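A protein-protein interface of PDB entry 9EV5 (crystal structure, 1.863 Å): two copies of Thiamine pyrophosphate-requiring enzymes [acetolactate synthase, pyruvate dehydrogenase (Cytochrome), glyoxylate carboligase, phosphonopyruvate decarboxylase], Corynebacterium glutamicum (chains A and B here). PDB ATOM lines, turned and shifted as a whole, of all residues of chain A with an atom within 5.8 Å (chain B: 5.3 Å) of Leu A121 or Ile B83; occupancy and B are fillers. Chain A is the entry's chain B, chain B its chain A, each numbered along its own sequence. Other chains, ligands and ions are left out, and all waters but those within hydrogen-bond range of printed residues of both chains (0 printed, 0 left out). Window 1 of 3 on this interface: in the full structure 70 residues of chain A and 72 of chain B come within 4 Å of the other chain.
OH of Tyr A87 is in hydrogen-bond range of OE1 of Glu A124.
Among the printed residues, pairs that only touch across the chains: Leu A121 with Leu B121 (3.6 Å), Thr A80 with Gln B84 (3.6 Å), Leu A121 with Ile B83 (3.7 Å), Ile A83 with Leu B121 (3.7 Å), Tyr A87 with Leu B121 (3.8 Å) and Leu A121 with Tyr B87 (3.8 Å).
Of the printed residues of chain B, Thr A80 touches Gln B84 (3.6 Å).
Of the printed residues of chain B, Ile A83 touches Leu B121 (3.7 Å).
Of the printed residues of chain B, Tyr A87 touches Leu B121 (3.8 Å).
Of chain B, only Ile B83 (3.7 Å), Tyr B87 (3.8 Å) and Leu B121 (3.6 Å) come within 4 Å of Leu A121.
Printed residues of chain A within 4 Å of Leu B121: Ile A83, Tyr A87 and Leu A121.
Of the 13 printed residues of chain A, 4 touch a printed residue of chain B.
Printed residues of chain A that touch a printed residue of chain B: Thr A80, Ile A83, Tyr A87 and Leu A121.
Hydrophobic or aromatic side chains of chain A within 4 Å of the printed part of chain B: Ile A83, Tyr A87 and Leu A121.
Of the 13 printed residues of chain B, 4 touch a printed residue of chain A.
Printed residues of chain B that touch a printed residue of chain A: Ile B83, Gln B84, Tyr B87 and Leu B121.
Along chain B the printed residues that touch a printed residue of chain A span positions 83 to 121.
Among the printed residues, 6 pairs touch across the chains.
Among the printed residues, no Asp or Glu carboxylate lies within 4 Å of a Lys or Arg side-chain nitrogen of the other chain.
Ile A83 touches Leu B121, and with the chains exchanged Leu A121 touches Ile B83.
Tyr A87 touches Leu B121, and with the chains exchanged Leu A121 touches Tyr B87.
Leu A121 touches its own counterpart, Leu B121.
Positions printed for both chains: 79, 80, 83, 87, 121, 122 and 125.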
ATOM      1  N   ASN A  79     -17.429   3.127  21.855  1.00  0.00           N
ATOM      2  CA  ASN A  79     -17.967   2.550  23.080  1.00  0.00           C
ATOM      3  C   ASN A  79     -18.377   1.087  22.898  1.00  0.00           C
ATOM      4  O   ASN A  79     -18.306   0.331  23.859  1.00  0.00           O
ATOM      5  CB  ASN A  79     -19.073   3.402  23.680  1.00  0.00           C
ATOM      6  CG  ASN A  79     -20.337   3.390  22.889  1.00  0.00           C
ATOM      7  OD1 ASN A  79     -21.014   2.360  22.751  1.00  0.00           O
ATOM      8  ND2 ASN A  79     -20.689   4.534  22.358  1.00  0.00           N
ATOM      9  N   THR A  80     -18.755   0.668  21.668  1.00  0.00           N
ATOM     10  CA  THR A  80     -19.123  -0.728  21.384  1.00  0.00           C
ATOM     11  C   THR A  80     -17.983  -1.687  21.792  1.00  0.00           C
ATOM     12  O   THR A  80     -18.241  -2.742  22.397  1.00  0.00           O
ATOM     13  CB  THR A  80     -19.567  -0.877  19.912  1.00  0.00           C
ATOM     14  OG1 THR A  80     -20.703  -0.040  19.685  1.00  0.00           O
ATOM     15  CG2 THR A  80     -19.975  -2.282  19.554  1.00  0.00           C
ATOM     16  N   ILE A  83     -17.605  -3.404  25.561  1.00  0.00           N
ATOM     17  CA  ILE A  83     -18.530  -4.446  25.990  1.00  0.00           C
ATOM     18  C   ILE A  83     -17.891  -5.715  26.635  1.00  0.00           C
ATOM     19  O   ILE A  83     -18.327  -6.063  27.730  1.00  0.00           O
ATOM     20  CB  ILE A  83     -19.541  -4.827  24.898  1.00  0.00           C
ATOM     21  CG1 ILE A  83     -20.751  -5.509  25.541  1.00  0.00           C
ATOM     22  CG2 ILE A  83     -18.926  -5.632  23.723  1.00  0.00           C
ATOM     23  CD1 ILE A  83     -22.074  -5.207  24.838  1.00  0.00           C
ATOM     24  N   TYR A  87     -18.619  -6.630  30.587  1.00  0.00           N
ATOM     25  CA  TYR A  87     -19.225  -7.889  31.083  1.00  0.00           C
ATOM     26  C   TYR A  87     -18.314  -8.499  32.136  1.00  0.00           C
ATOM     27  O   TYR A  87     -18.793  -8.947  33.166  1.00  0.00           O
ATOM     28  CB  TYR A  87     -19.387  -8.911  29.953  1.00  0.00           C
ATOM     29  CG  TYR A  87     -20.733  -8.875  29.268  1.00  0.00           C
ATOM     30  CD1 TYR A  87     -21.849  -9.467  29.851  1.00  0.00           C
ATOM     31  CD2 TYR A  87     -20.877  -8.307  28.007  1.00  0.00           C
ATOM     32  CE1 TYR A  87     -23.080  -9.457  29.212  1.00  0.00           C
ATOM     33  CE2 TYR A  87     -22.098  -8.302  27.356  1.00  0.00           C
ATOM     34  CZ  TYR A  87     -23.203  -8.857  27.972  1.00  0.00           C
ATOM     35  OH  TYR A  87     -24.413  -8.836  27.338  1.00  0.00           O
ATOM     36  N   HIS A 117     -27.300   2.408  19.905  1.00  0.00           N
ATOM     37  CA  HIS A 117     -28.062   2.793  21.082  1.00  0.00           C
ATOM     38  C   HIS A 117     -27.366   2.140  22.269  1.00  0.00           C
ATOM     39  O   HIS A 117     -27.788   1.058  22.710  1.00  0.00           O
ATOM     40  CB  HIS A 117     -29.520   2.281  20.961  1.00  0.00           C
ATOM     41  CG  HIS A 117     -30.357   3.050  19.991  1.00  0.00           C
ATOM     42  ND1 HIS A 117     -30.245   2.854  18.629  1.00  0.00           N
ATOM     43  CD2 HIS A 117     -31.307   3.992  20.221  1.00  0.00           C
ATOM     44  CE1 HIS A 117     -31.146   3.645  18.072  1.00  0.00           C
ATOM     45  NE2 HIS A 117     -31.820   4.343  18.996  1.00  0.00           N
ATOM     46  N   PRO A 118     -26.250   2.734  22.760  1.00  0.00           N
ATOM     47  CA  PRO A 118     -25.527   2.110  23.893  1.00  0.00           C
ATOM     48  C   PRO A 118     -26.374   1.985  25.148  1.00  0.00           C
ATOM     49  O   PRO A 118     -26.228   1.018  25.880  1.00  0.00           O
ATOM     50  CB  PRO A 118     -24.337   3.031  24.152  1.00  0.00           C
ATOM     51  CG  PRO A 118     -24.333   4.033  23.060  1.00  0.00           C
ATOM     52  CD  PRO A 118     -25.651   4.024  22.353  1.00  0.00           C
ATOM     53  N   GLU A 119     -27.305   2.934  25.366  1.00  0.00           N
ATOM     54  CA  GLU A 119     -28.216   2.906  26.504  1.00  0.00           C
ATOM     55  C   GLU A 119     -29.086   1.626  26.530  1.00  0.00           C
ATOM     56  O   GLU A 119     -29.566   1.237  27.596  1.00  0.00           O
ATOM     57  CB  GLU A 119     -29.055   4.213  26.577  1.00  0.00           C
ATOM     58  CG  GLU A 119     -30.052   4.402  25.440  1.00  0.00           C
ATOM     59  CD  GLU A 119     -29.560   4.890  24.077  1.00  0.00           C
ATOM     60  OE1 GLU A 119     -28.330   5.051  23.884  1.00  0.00           O
ATOM     61  OE2 GLU A 119     -30.419   5.088  23.183  1.00  0.00           O
ATOM     62  N   ILE A 120     -29.237   0.939  25.379  1.00  0.00           N
ATOM     63  CA  ILE A 120     -29.964  -0.323  25.279  1.00  0.00           C
ATOM     64  C   ILE A 120     -28.976  -1.503  25.290  1.00  0.00           C
ATOM     65  O   ILE A 120     -29.156  -2.479  26.038  1.00  0.00           O
ATOM     66  CB  ILE A 120     -30.845  -0.352  24.011  1.00  0.00           C
ATOM     67  CG1 ILE A 120     -31.882   0.767  24.054  1.00  0.00           C
ATOM     68  CG2 ILE A 120     -31.525  -1.724  23.849  1.00  0.00           C
ATOM     69  CD1 ILE A 120     -32.732   0.916  22.770  1.00  0.00           C
ATOM     70  N   LEU A 121     -27.919  -1.404  24.468  1.00  0.00           N
ATOM     71  CA  LEU A 121     -26.892  -2.425  24.328  1.00  0.00           C
ATOM     72  C   LEU A 121     -26.260  -2.842  25.654  1.00  0.00           C
ATOM     73  O   LEU A 121     -26.042  -4.041  25.860  1.00  0.00           O
ATOM     74  CB  LEU A 121     -25.790  -1.918  23.363  1.00  0.00           C
ATOM     75  CG  LEU A 121     -24.773  -2.980  22.923  1.00  0.00           C
ATOM     76  CD1 LEU A 121     -25.450  -4.065  22.090  1.00  0.00           C
ATOM     77  CD2 LEU A 121     -23.589  -2.344  22.154  1.00  0.00           C
ATOM     78  N   PHE A 122     -25.945  -1.885  26.548  1.00  0.00           N
ATOM     79  CA  PHE A 122     -25.207  -2.224  27.777  1.00  0.00           C
ATOM     80  C   PHE A 122     -26.046  -2.648  28.974  1.00  0.00           C
ATOM     81  O   PHE A 122     -25.489  -2.786  30.052  1.00  0.00           O
ATOM     82  CB  PHE A 122     -24.280  -1.066  28.200  1.00  0.00           C
ATOM     83  CG  PHE A 122     -23.186  -0.779  27.208  1.00  0.00           C
ATOM     84  CD1 PHE A 122     -22.335  -1.784  26.780  1.00  0.00           C
ATOM     85  CD2 PHE A 122     -22.997   0.494  26.708  1.00  0.00           C
ATOM     86  CE1 PHE A 122     -21.320  -1.515  25.873  1.00  0.00           C
ATOM     87  CE2 PHE A 122     -21.987   0.752  25.795  1.00  0.00           C
ATOM     88  CZ  PHE A 122     -21.158  -0.245  25.387  1.00  0.00           C
ATOM     89  N   LYS A 123     -27.355  -2.839  28.815  1.00  0.00           N
ATOM     90  CA  LYS A 123     -28.221  -3.212  29.942  1.00  0.00           C
ATOM     91  C   LYS A 123     -27.780  -4.487  30.660  1.00  0.00           C
ATOM     92  O   LYS A 123     -27.854  -4.534  31.889  1.00  0.00           O
ATOM     93  CB  LYS A 123     -29.699  -3.328  29.516  1.00  0.00           C
ATOM     94  CG  LYS A 123     -30.343  -2.030  29.022  1.00  0.00           C
ATOM     95  CD  LYS A 123     -30.413  -0.950  30.088  1.00  0.00           C
ATOM     96  CE  LYS A 123     -31.617  -0.043  29.917  1.00  0.00           C
ATOM     97  NZ  LYS A 123     -31.246   1.416  29.884  1.00  0.00           N
ATOM     98  N   GLU A 124     -27.365  -5.534  29.915  1.00  0.00           N
ATOM     99  CA  GLU A 124     -26.992  -6.797  30.558  1.00  0.00           C
ATOM    100  C   GLU A 124     -25.661  -6.742  31.306  1.00  0.00           C
ATOM    101  O   GLU A 124     -25.514  -7.411  32.329  1.00  0.00           O
ATOM    102  CB  GLU A 124     -27.008  -7.971  29.570  1.00  0.00           C
ATOM    103  CG  GLU A 124     -26.796  -9.318  30.256  1.00  0.00           C
ATOM    104  CD  GLU A 124     -26.696 -10.546  29.376  1.00  0.00           C
ATOM    105  OE1 GLU A 124     -26.341 -10.411  28.178  1.00  0.00           O
ATOM    106  OE2 GLU A 124     -26.975 -11.653  29.893  1.00  0.00           O
ATOM    107  N   CYS A 125     -24.713  -5.930  30.844  1.00  0.00           N
ATOM    108  CA  CYS A 125     -23.415  -5.853  31.504  1.00  0.00           C
ATOM    109  C   CYS A 125     -23.314  -4.668  32.466  1.00  0.00           C
ATOM    110  O   CYS A 125     -22.206  -4.145  32.661  1.00  0.00           O
ATOM    111  CB  CYS A 125     -22.291  -5.844  30.474  1.00  0.00           C
ATOM    112  SG  CYS A 125     -22.383  -4.454  29.309  1.00  0.00           S
ATOM    113  N   ASN B  79     -18.973 -15.222  21.195  1.00  0.00           N
ATOM    114  CA  ASN B  79     -19.867 -14.535  20.281  1.00  0.00           C
ATOM    115  C   ASN B  79     -19.952 -13.051  20.584  1.00  0.00           C
ATOM    116  O   ASN B  79     -20.203 -12.274  19.669  1.00  0.00           O
ATOM    117  CB  ASN B  79     -21.226 -15.202  20.196  1.00  0.00           C
ATOM    118  CG  ASN B  79     -22.063 -15.056  21.440  1.00  0.00           C
ATOM    119  OD1 ASN B  79     -22.470 -13.951  21.809  1.00  0.00           O
ATOM    120  ND2 ASN B  79     -22.354 -16.180  22.094  1.00  0.00           N
ATOM    121  N   THR B  80     -19.694 -12.629  21.846  1.00  0.00           N
ATOM    122  CA  THR B  80     -19.726 -11.195  22.206  1.00  0.00           C
ATOM    123  C   THR B  80     -18.720 -10.418  21.345  1.00  0.00           C
ATOM    124  O   THR B  80     -19.030  -9.324  20.898  1.00  0.00           O
ATOM    125  CB  THR B  80     -19.470 -11.041  23.726  1.00  0.00           C
ATOM    126  OG1 THR B  80     -20.525 -11.700  24.443  1.00  0.00           O
ATOM    127  CG2 THR B  80     -19.407  -9.588  24.184  1.00  0.00           C
ATOM    128  N   HIS B  81     -17.549 -11.044  21.012  1.00  0.00           N
ATOM    129  CA  HIS B  81     -16.537 -10.428  20.172  1.00  0.00           C
ATOM    130  C   HIS B  81     -16.990 -10.152  18.735  1.00  0.00           C
ATOM    131  O   HIS B  81     -16.432  -9.262  18.110  1.00  0.00           O
ATOM    132  CB  HIS B  81     -15.261 -11.264  20.138  1.00  0.00           C
ATOM    133  CG  HIS B  81     -14.238 -10.859  21.137  1.00  0.00           C
ATOM    134  ND1 HIS B  81     -13.235 -11.741  21.530  1.00  0.00           N
ATOM    135  CD2 HIS B  81     -14.065  -9.678  21.781  1.00  0.00           C
ATOM    136  CE1 HIS B  81     -12.490 -11.071  22.398  1.00  0.00           C
ATOM    137  NE2 HIS B  81     -12.950  -9.824  22.578  1.00  0.00           N
ATOM    138  N   LEU B  82     -18.004 -10.873  18.220  1.00  0.00           N
ATOM    139  CA  LEU B  82     -18.503 -10.647  16.865  1.00  0.00           C
ATOM    140  C   LEU B  82     -19.106  -9.259  16.666  1.00  0.00           C
ATOM    141  O   LEU B  82     -19.124  -8.780  15.557  1.00  0.00           O
ATOM    142  CB  LEU B  82     -19.640 -11.650  16.548  1.00  0.00           C
ATOM    143  CG  LEU B  82     -19.250 -13.163  16.518  1.00  0.00           C
ATOM    144  CD1 LEU B  82     -20.501 -14.041  16.376  1.00  0.00           C
ATOM    145  CD2 LEU B  82     -18.237 -13.448  15.371  1.00  0.00           C
ATOM    146  N   ILE B  83     -19.678  -8.671  17.716  1.00  0.00           N
ATOM    147  CA  ILE B  83     -20.541  -7.498  17.686  1.00  0.00           C
ATOM    148  C   ILE B  83     -20.058  -6.317  16.790  1.00  0.00           C
ATOM    149  O   ILE B  83     -20.873  -5.861  15.990  1.00  0.00           O
ATOM    150  CB  ILE B  83     -20.928  -7.022  19.114  1.00  0.00           C
ATOM    151  CG1 ILE B  83     -22.153  -6.092  19.057  1.00  0.00           C
ATOM    152  CG2 ILE B  83     -19.762  -6.356  19.840  1.00  0.00           C
ATOM    153  CD1 ILE B  83     -23.092  -6.252  20.215  1.00  0.00           C
ATOM    154  N   GLN B  84     -18.784  -5.871  16.851  1.00  0.00           N
ATOM    155  CA  GLN B  84     -18.346  -4.723  16.031  1.00  0.00           C
ATOM    156  C   GLN B  84     -18.481  -5.042  14.534  1.00  0.00           C
ATOM    157  O   GLN B  84     -18.938  -4.195  13.753  1.00  0.00           O
ATOM    158  CB  GLN B  84     -16.876  -4.337  16.346  1.00  0.00           C
ATOM    159  CG  GLN B  84     -16.462  -2.980  15.709  1.00  0.00           C
ATOM    160  CD  GLN B  84     -16.928  -1.828  16.586  1.00  0.00           C
ATOM    161  OE1 GLN B  84     -18.110  -1.419  16.585  1.00  0.00           O
ATOM    162  NE2 GLN B  84     -16.004  -1.283  17.363  1.00  0.00           N
ATOM    163  N   GLY B  85     -18.082  -6.263  14.166  1.00  0.00           N
ATOM    164  CA  GLY B  85     -18.113  -6.716  12.792  1.00  0.00           C
ATOM    165  C   GLY B  85     -19.514  -6.917  12.273  1.00  0.00           C
ATOM    166  O   GLY B  85     -19.772  -6.646  11.091  1.00  0.00           O
ATOM    167  N   LEU B  86     -20.439  -7.354  13.159  1.00  0.00           N
ATOM    168  CA  LEU B  86     -21.832  -7.515  12.795  1.00  0.00           C
ATOM    169  C   LEU B  86     -22.499  -6.152  12.585  1.00  0.00           C
ATOM    170  O   LEU B  86     -23.279  -6.020  11.644  1.00  0.00           O
ATOM    171  CB  LEU B  86     -22.608  -8.383  13.808  1.00  0.00           C
ATOM    172  CG  LEU B  86     -22.111  -9.835  13.965  1.00  0.00           C
ATOM    173  CD1 LEU B  86     -23.058 -10.609  14.835  1.00  0.00           C
ATOM    174  CD2 LEU B  86     -21.922 -10.537  12.597  1.00  0.00           C
ATOM    175  N   TYR B  87     -22.188  -5.118  13.411  1.00  0.00           N
ATOM    176  CA  TYR B  87     -22.780  -3.773  13.177  1.00  0.00           C
ATOM    177  C   TYR B  87     -22.297  -3.251  11.819  1.00  0.00           C
ATOM    178  O   TYR B  87     -23.083  -2.682  11.066  1.00  0.00           O
ATOM    179  CB  TYR B  87     -22.334  -2.755  14.249  1.00  0.00           C
ATOM    180  CG  TYR B  87     -23.250  -2.609  15.444  1.00  0.00           C
ATOM    181  CD1 TYR B  87     -24.401  -1.828  15.377  1.00  0.00           C
ATOM    182  CD2 TYR B  87     -22.944  -3.215  16.657  1.00  0.00           C
ATOM    183  CE1 TYR B  87     -25.251  -1.700  16.472  1.00  0.00           C
ATOM    184  CE2 TYR B  87     -23.784  -3.092  17.758  1.00  0.00           C
ATOM    185  CZ  TYR B  87     -24.935  -2.332  17.662  1.00  0.00           C
ATOM    186  OH  TYR B  87     -25.749  -2.191  18.762  1.00  0.00           O
ATOM    187  N   ASP B  88     -21.004  -3.474  11.485  1.00  0.00           N
ATOM    188  CA  ASP B  88     -20.467  -2.995  10.224  1.00  0.00           C
ATOM    189  C   ASP B  88     -21.088  -3.749   9.022  1.00  0.00           C
ATOM    190  O   ASP B  88     -21.466  -3.123   8.049  1.00  0.00           O
ATOM    191  CB  ASP B  88     -18.928  -3.139  10.196  1.00  0.00           C
ATOM    192  CG  ASP B  88     -18.365  -2.544   8.922  1.00  0.00           C
ATOM    193  OD1 ASP B  88     -18.473  -1.313   8.748  1.00  0.00           O
ATOM    194  OD2 ASP B  88     -17.908  -3.312   8.073  1.00  0.00           O
ATOM    195  N   LEU B 121     -28.848  -9.207  22.912  1.00  0.00           N
ATOM    196  CA  LEU B 121     -27.711  -8.358  22.614  1.00  0.00           C
ATOM    197  C   LEU B 121     -27.616  -7.971  21.133  1.00  0.00           C
ATOM    198  O   LEU B 121     -27.337  -6.826  20.835  1.00  0.00           O
ATOM    199  CB  LEU B 121     -26.391  -9.075  23.051  1.00  0.00           C
ATOM    200  CG  LEU B 121     -25.117  -8.199  23.024  1.00  0.00           C
ATOM    201  CD1 LEU B 121     -25.218  -7.093  24.051  1.00  0.00           C
ATOM    202  CD2 LEU B 121     -23.872  -9.024  23.316  1.00  0.00           C
ATOM    203  N   PHE B 122     -27.824  -8.918  20.218  1.00  0.00           N
ATOM    204  CA  PHE B 122     -27.646  -8.651  18.780  1.00  0.00           C
ATOM    205  C   PHE B 122     -28.859  -8.095  18.027  1.00  0.00           C
ATOM    206  O   PHE B 122     -28.779  -7.993  16.805  1.00  0.00           O
ATOM    207  CB  PHE B 122     -27.151  -9.908  18.061  1.00  0.00           C
ATOM    208  CG  PHE B 122     -25.790 -10.378  18.526  1.00  0.00           C
ATOM    209  CD1 PHE B 122     -24.711  -9.514  18.553  1.00  0.00           C
ATOM    210  CD2 PHE B 122     -25.593 -11.687  18.947  1.00  0.00           C
ATOM    211  CE1 PHE B 122     -23.442  -9.963  18.954  1.00  0.00           C
ATOM    212  CE2 PHE B 122     -24.334 -12.120  19.375  1.00  0.00           C
ATOM    213  CZ  PHE B 122     -23.277 -11.248  19.393  1.00  0.00           C
ATOM    214  N   CYS B 125     -27.883  -4.946  15.752  1.00  0.00           N
ATOM    215  CA  CYS B 125     -26.993  -5.166  14.607  1.00  0.00           C
ATOM    216  C   CYS B 125     -27.469  -6.315  13.708  1.00  0.00           C
ATOM    217  O   CYS B 125     -26.632  -6.996  13.113  1.00  0.00           O
ATOM    218  CB  CYS B 125     -25.562  -5.385  15.085  1.00  0.00           C
ATOM    219  SG  CYS B 125     -25.368  -6.795  16.215  1.00  0.00           S
